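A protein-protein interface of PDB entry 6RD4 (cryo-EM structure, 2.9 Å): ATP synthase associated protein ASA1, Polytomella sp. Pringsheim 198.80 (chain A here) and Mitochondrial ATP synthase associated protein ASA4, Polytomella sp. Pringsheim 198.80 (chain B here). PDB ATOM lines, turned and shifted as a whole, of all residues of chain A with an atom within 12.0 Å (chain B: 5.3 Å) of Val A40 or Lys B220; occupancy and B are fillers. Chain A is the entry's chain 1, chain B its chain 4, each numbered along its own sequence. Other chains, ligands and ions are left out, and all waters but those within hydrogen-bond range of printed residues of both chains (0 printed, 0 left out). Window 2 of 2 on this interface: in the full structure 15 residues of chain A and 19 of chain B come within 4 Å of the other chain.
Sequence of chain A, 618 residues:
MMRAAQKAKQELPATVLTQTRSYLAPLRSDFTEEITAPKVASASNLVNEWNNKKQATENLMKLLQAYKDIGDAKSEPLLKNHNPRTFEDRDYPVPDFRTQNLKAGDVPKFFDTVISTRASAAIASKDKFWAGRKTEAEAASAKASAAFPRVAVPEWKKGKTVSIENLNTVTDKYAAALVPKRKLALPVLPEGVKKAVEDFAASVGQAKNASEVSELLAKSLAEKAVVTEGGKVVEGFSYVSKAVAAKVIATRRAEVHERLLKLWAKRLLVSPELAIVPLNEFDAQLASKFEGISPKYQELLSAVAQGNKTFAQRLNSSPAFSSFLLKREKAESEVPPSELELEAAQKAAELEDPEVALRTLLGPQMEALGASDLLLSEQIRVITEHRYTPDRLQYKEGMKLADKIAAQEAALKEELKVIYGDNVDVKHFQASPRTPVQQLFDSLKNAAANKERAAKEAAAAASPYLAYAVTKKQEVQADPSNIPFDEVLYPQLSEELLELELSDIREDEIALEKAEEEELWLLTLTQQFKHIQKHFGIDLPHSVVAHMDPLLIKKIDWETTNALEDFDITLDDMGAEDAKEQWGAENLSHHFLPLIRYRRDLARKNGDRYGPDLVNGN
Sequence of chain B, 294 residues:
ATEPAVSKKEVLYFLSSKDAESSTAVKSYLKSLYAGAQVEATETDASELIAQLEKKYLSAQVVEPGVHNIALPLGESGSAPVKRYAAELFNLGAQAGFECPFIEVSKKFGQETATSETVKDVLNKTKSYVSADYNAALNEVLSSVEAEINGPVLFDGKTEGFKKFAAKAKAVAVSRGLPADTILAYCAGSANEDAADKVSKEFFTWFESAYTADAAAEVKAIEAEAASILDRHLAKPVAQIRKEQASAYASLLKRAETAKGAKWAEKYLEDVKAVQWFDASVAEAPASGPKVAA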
ATOM      1  N   THR A  36       2.579 -29.717   6.596  1.00  0.00           N
ATOM      2  CA  THR A  36       2.754 -30.526   7.784  1.00  0.00           C
ATOM      3  C   THR A  36       2.342 -29.753   9.021  1.00  0.00           C
ATOM      4  O   THR A  36       1.996 -28.576   8.966  1.00  0.00           O
ATOM      5  CB  THR A  36       4.202 -30.990   7.921  1.00  0.00           C
ATOM      6  OG1 THR A  36       5.071 -29.864   7.778  1.00  0.00           O
ATOM      7  CG2 THR A  36       4.539 -32.035   6.896  1.00  0.00           C
ATOM      8  N   ALA A  37       2.347 -30.462  10.137  1.00  0.00           N
ATOM      9  CA  ALA A  37       2.192 -29.837  11.429  1.00  0.00           C
ATOM     10  C   ALA A  37       3.508 -29.168  11.815  1.00  0.00           C
ATOM     11  O   ALA A  37       4.578 -29.613  11.399  1.00  0.00           O
ATOM     12  CB  ALA A  37       1.788 -30.881  12.464  1.00  0.00           C
ATOM     13  N   PRO A  38       3.464 -28.090  12.596  1.00  0.00           N
ATOM     14  CA  PRO A  38       4.659 -27.258  12.739  1.00  0.00           C
ATOM     15  C   PRO A  38       5.702 -27.673  13.769  1.00  0.00           C
ATOM     16  O   PRO A  38       6.539 -26.826  14.093  1.00  0.00           O
ATOM     17  CB  PRO A  38       4.072 -25.895  13.108  1.00  0.00           C
ATOM     18  CG  PRO A  38       2.652 -25.982  12.847  1.00  0.00           C
ATOM     19  CD  PRO A  38       2.277 -27.369  13.068  1.00  0.00           C
ATOM     20  N   LYS A  39       5.683 -28.910  14.282  1.00  0.00           N
ATOM     21  CA  LYS A  39       6.745 -29.494  15.123  1.00  0.00           C
ATOM     22  C   LYS A  39       6.959 -28.723  16.433  1.00  0.00           C
ATOM     23  O   LYS A  39       7.964 -28.044  16.625  1.00  0.00           O
ATOM     24  CB  LYS A  39       8.072 -29.595  14.364  1.00  0.00           C
ATOM     25  CG  LYS A  39       8.148 -30.722  13.378  1.00  0.00           C
ATOM     26  CD  LYS A  39       8.188 -32.063  14.067  1.00  0.00           C
ATOM     27  CE  LYS A  39       8.107 -33.190  13.059  1.00  0.00           C
ATOM     28  NZ  LYS A  39       6.815 -33.181  12.320  1.00  0.00           N
ATOM     29  N   VAL A  40       5.974 -28.840  17.325  1.00  0.00           N
ATOM     30  CA  VAL A  40       6.072 -28.255  18.662  1.00  0.00           C
ATOM     31  C   VAL A  40       7.208 -28.907  19.435  1.00  0.00           C
ATOM     32  O   VAL A  40       7.212 -30.123  19.646  1.00  0.00           O
ATOM     33  CB  VAL A  40       4.754 -28.415  19.413  1.00  0.00           C
ATOM     34  CG1 VAL A  40       4.881 -27.896  20.809  1.00  0.00           C
ATOM     35  CG2 VAL A  40       3.653 -27.694  18.703  1.00  0.00           C
ATOM     36  N   ALA A  41       8.177 -28.102  19.867  1.00  0.00           N
ATOM     37  CA  ALA A  41       9.303 -28.613  20.632  1.00  0.00           C
ATOM     38  C   ALA A  41       8.893 -28.900  22.067  1.00  0.00           C
ATOM     39  O   ALA A  41       7.820 -28.513  22.528  1.00  0.00           O
ATOM     40  CB  ALA A  41      10.467 -27.629  20.625  1.00  0.00           C
ATOM     41  N   SER A  42       9.773 -29.587  22.776  1.00  0.00           N
ATOM     42  CA  SER A  42       9.462 -30.095  24.100  1.00  0.00           C
ATOM     43  C   SER A  42       9.718 -29.041  25.163  1.00  0.00           C
ATOM     44  O   SER A  42      10.498 -28.108  24.973  1.00  0.00           O
ATOM     45  CB  SER A  42      10.292 -31.338  24.388  1.00  0.00           C
ATOM     46  OG  SER A  42      11.622 -31.142  23.948  1.00  0.00           O
ATOM     47  N   ALA A  43       9.049 -29.211  26.297  1.00  0.00           N
ATOM     48  CA  ALA A  43       9.214 -28.296  27.414  1.00  0.00           C
ATOM     49  C   ALA A  43      10.595 -28.478  28.014  1.00  0.00           C
ATOM     50  O   ALA A  43      10.909 -29.541  28.555  1.00  0.00           O
ATOM     51  CB  ALA A  43       8.142 -28.542  28.467  1.00  0.00           C
ATOM     52  N   SER A  44      11.429 -27.453  27.888  1.00  0.00           N
ATOM     53  CA  SER A  44      12.775 -27.526  28.419  1.00  0.00           C
ATOM     54  C   SER A  44      12.732 -27.453  29.932  1.00  0.00           C
ATOM     55  O   SER A  44      11.895 -26.767  30.516  1.00  0.00           O
ATOM     56  CB  SER A  44      13.625 -26.393  27.855  1.00  0.00           C
ATOM     57  OG  SER A  44      15.002 -26.652  28.033  1.00  0.00           O
ATOM     58  N   LYS A 158       5.612  -7.507  33.846  1.00  0.00           N
ATOM     59  CA  LYS A 158       5.669  -8.338  32.645  1.00  0.00           C
ATOM     60  C   LYS A 158       5.904  -7.511  31.391  1.00  0.00           C
ATOM     61  O   LYS A 158       6.838  -7.769  30.627  1.00  0.00           O
ATOM     62  CB  LYS A 158       4.392  -9.155  32.514  1.00  0.00           C
ATOM     63  CG  LYS A 158       4.406 -10.137  31.370  1.00  0.00           C
ATOM     64  CD  LYS A 158       5.454 -11.178  31.558  1.00  0.00           C
ATOM     65  CE  LYS A 158       5.021 -12.505  31.007  1.00  0.00           C
ATOM     66  NZ  LYS A 158       3.812 -13.030  31.661  1.00  0.00           N
ATOM     67  N   ALA B 215      -3.273 -21.457  12.375  1.00  0.00           N
ATOM     68  CA  ALA B 215      -2.477 -20.342  12.847  1.00  0.00           C
ATOM     69  C   ALA B 215      -2.091 -20.537  14.295  1.00  0.00           C
ATOM     70  O   ALA B 215      -0.950 -20.273  14.672  1.00  0.00           O
ATOM     71  CB  ALA B 215      -3.239 -19.040  12.671  1.00  0.00           C
ATOM     72  N   ALA B 216      -3.012 -21.033  15.117  1.00  0.00           N
ATOM     73  CA  ALA B 216      -2.704 -21.226  16.524  1.00  0.00           C
ATOM     74  C   ALA B 216      -1.756 -22.383  16.736  1.00  0.00           C
ATOM     75  O   ALA B 216      -1.054 -22.416  17.741  1.00  0.00           O
ATOM     76  CB  ALA B 216      -3.973 -21.450  17.331  1.00  0.00           C
ATOM     77  N   ALA B 217      -1.720 -23.339  15.823  1.00  0.00           N
ATOM     78  CA  ALA B 217      -0.704 -24.373  15.897  1.00  0.00           C
ATOM     79  C   ALA B 217       0.638 -23.882  15.407  1.00  0.00           C
ATOM     80  O   ALA B 217       1.656 -24.493  15.719  1.00  0.00           O
ATOM     81  CB  ALA B 217      -1.115 -25.587  15.085  1.00  0.00           C
ATOM     82  N   GLU B 218       0.654 -22.823  14.611  1.00  0.00           N
ATOM     83  CA  GLU B 218       1.904 -22.226  14.171  1.00  0.00           C
ATOM     84  C   GLU B 218       2.483 -21.324  15.236  1.00  0.00           C
ATOM     85  O   GLU B 218       3.699 -21.233  15.376  1.00  0.00           O
ATOM     86  CB  GLU B 218       1.668 -21.441  12.886  1.00  0.00           C
ATOM     87  CG  GLU B 218       2.913 -20.951  12.230  1.00  0.00           C
ATOM     88  CD  GLU B 218       3.779 -22.075  11.730  1.00  0.00           C
ATOM     89  OE1 GLU B 218       3.327 -22.798  10.816  1.00  0.00           O
ATOM     90  OE2 GLU B 218       4.906 -22.238  12.252  1.00  0.00           O
ATOM     91  N   VAL B 219       1.621 -20.648  15.984  1.00  0.00           N
ATOM     92  CA  VAL B 219       2.049 -19.820  17.098  1.00  0.00           C
ATOM     93  C   VAL B 219       2.549 -20.684  18.239  1.00  0.00           C
ATOM     94  O   VAL B 219       3.584 -20.398  18.833  1.00  0.00           O
ATOM     95  CB  VAL B 219       0.881 -18.922  17.523  1.00  0.00           C
ATOM     96  CG1 VAL B 219       1.157 -18.237  18.809  1.00  0.00           C
ATOM     97  CG2 VAL B 219       0.610 -17.943  16.453  1.00  0.00           C
ATOM     98  N   LYS B 220       1.866 -21.790  18.522  1.00  0.00           N
ATOM     99  CA  LYS B 220       2.294 -22.677  19.596  1.00  0.00           C
ATOM    100  C   LYS B 220       3.561 -23.438  19.267  1.00  0.00           C
ATOM    101  O   LYS B 220       4.111 -24.086  20.151  1.00  0.00           O
ATOM    102  CB  LYS B 220       1.202 -23.678  19.940  1.00  0.00           C
ATOM    103  CG  LYS B 220       0.053 -23.093  20.709  1.00  0.00           C
ATOM    104  CD  LYS B 220       0.504 -22.438  21.991  1.00  0.00           C
ATOM    105  CE  LYS B 220      -0.624 -21.640  22.613  1.00  0.00           C
ATOM    106  NZ  LYS B 220      -0.273 -21.132  23.960  1.00  0.00           N
ATOM    107  N   ALA B 221       4.022 -23.406  18.031  1.00  0.00           N
ATOM    108  CA  ALA B 221       5.312 -23.981  17.713  1.00  0.00           C
ATOM    109  C   ALA B 221       6.422 -22.959  17.722  1.00  0.00           C
ATOM    110  O   ALA B 221       7.578 -23.327  17.906  1.00  0.00           O
ATOM    111  CB  ALA B 221       5.274 -24.641  16.348  1.00  0.00           C
ATOM    112  N   ILE B 222       6.104 -21.693  17.475  1.00  0.00           N
ATOM    113  CA  ILE B 222       7.088 -20.631  17.615  1.00  0.00           C
ATOM    114  C   ILE B 222       7.293 -20.308  19.080  1.00  0.00           C
ATOM    115  O   ILE B 222       8.407 -20.023  19.518  1.00  0.00           O
ATOM    116  CB  ILE B 222       6.645 -19.398  16.807  1.00  0.00           C
ATOM    117  CG1 ILE B 222       6.619 -19.718  15.329  1.00  0.00           C
ATOM    118  CG2 ILE B 222       7.566 -18.253  16.998  1.00  0.00           C
ATOM    119  CD1 ILE B 222       7.928 -20.182  14.803  1.00  0.00           C
ATOM    120  N   GLU B 223       6.225 -20.379  19.865  1.00  0.00           N
ATOM    121  CA  GLU B 223       6.332 -20.217  21.304  1.00  0.00           C
ATOM    122  C   GLU B 223       7.157 -21.325  21.925  1.00  0.00           C
ATOM    123  O   GLU B 223       7.913 -21.089  22.865  1.00  0.00           O
ATOM    124  CB  GLU B 223       4.951 -20.221  21.925  1.00  0.00           C
ATOM    125  CG  GLU B 223       4.181 -18.981  21.732  1.00  0.00           C
ATOM    126  CD  GLU B 223       2.875 -19.045  22.441  1.00  0.00           C
ATOM    127  OE1 GLU B 223       2.676 -20.008  23.193  1.00  0.00           O
ATOM    128  OE2 GLU B 223       2.042 -18.143  22.262  1.00  0.00           O
ATOM    129  N   ALA B 224       7.007 -22.540  21.431  1.00  0.00           N
ATOM    130  CA  ALA B 224       7.758 -23.658  21.968  1.00  0.00           C
ATOM    131  C   ALA B 224       9.183 -23.685  21.462  1.00  0.00           C
ATOM    132  O   ALA B 224      10.056 -24.220  22.136  1.00  0.00           O
ATOM    133  CB  ALA B 224       7.059 -24.959  21.619  1.00  0.00           C
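The side-chain carboxylate of Glu B223 lies within salt-bridge range of the side-chain amino group of Lys B220 (3.2 Å).
Among the printed residues, merely in contact across the chains: Pro A38 with Ala B217, Pro A38 with Glu B218, Pro A38 with Ala B221, Val A40 with Lys B220, Val A40 with Ala B224 and Ala A41 with Ala B224.
Val A40 touches two residues of chain B.
Lys B220 touches one residue of chain A.
Of chain A, only Pro A38 comes within 4 Å of Glu B218.
No residue of chain A comes within 4 Å of Val B219.
Of chain A, only Pro A38 comes within 4 Å of Ala B221.
No residue of chain A comes within 4 Å of Glu B223.
Ala B224 touches two residues of chain A.
Of the printed residues of chain B, Ala A41 touches Ala B224.
Printed residues of chain B within 4 Å of Pro A38: Ala B217 (3.4 Å), Glu B218 (3.8 Å) and Ala B221 (3.4 Å).
The nearest residue of chain A that does not touch Lys B220 is Ala A41 (5.7 Å).
The nearest printed residue of chain B that does not touch Pro A38 is Ile B222 (6.2 Å).
Of the 10 printed residues of chain A, 3 touch a printed residue of chain B.
Printed residues of chain A that touch a printed residue of chain B: Pro A38, Val A40 and Ala A41.
Hydrophobic or aromatic side chains of chain A within 4 Å of the printed part of chain B: Pro A38, Val A40 and Ala A41.
Of the 10 printed residues of chain B, 5 touch a printed residue of chain A.
Hydrophobic or aromatic side chains of chain B that line the printed part of chain A: Ala B221 and Ala B224.
Among the printed residues, 6 pairs touch across the chains.
Among the printed residues, no Asp or Glu carboxylate lies within 4 Å of a Lys or Arg side-chain nitrogen of the other chain.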
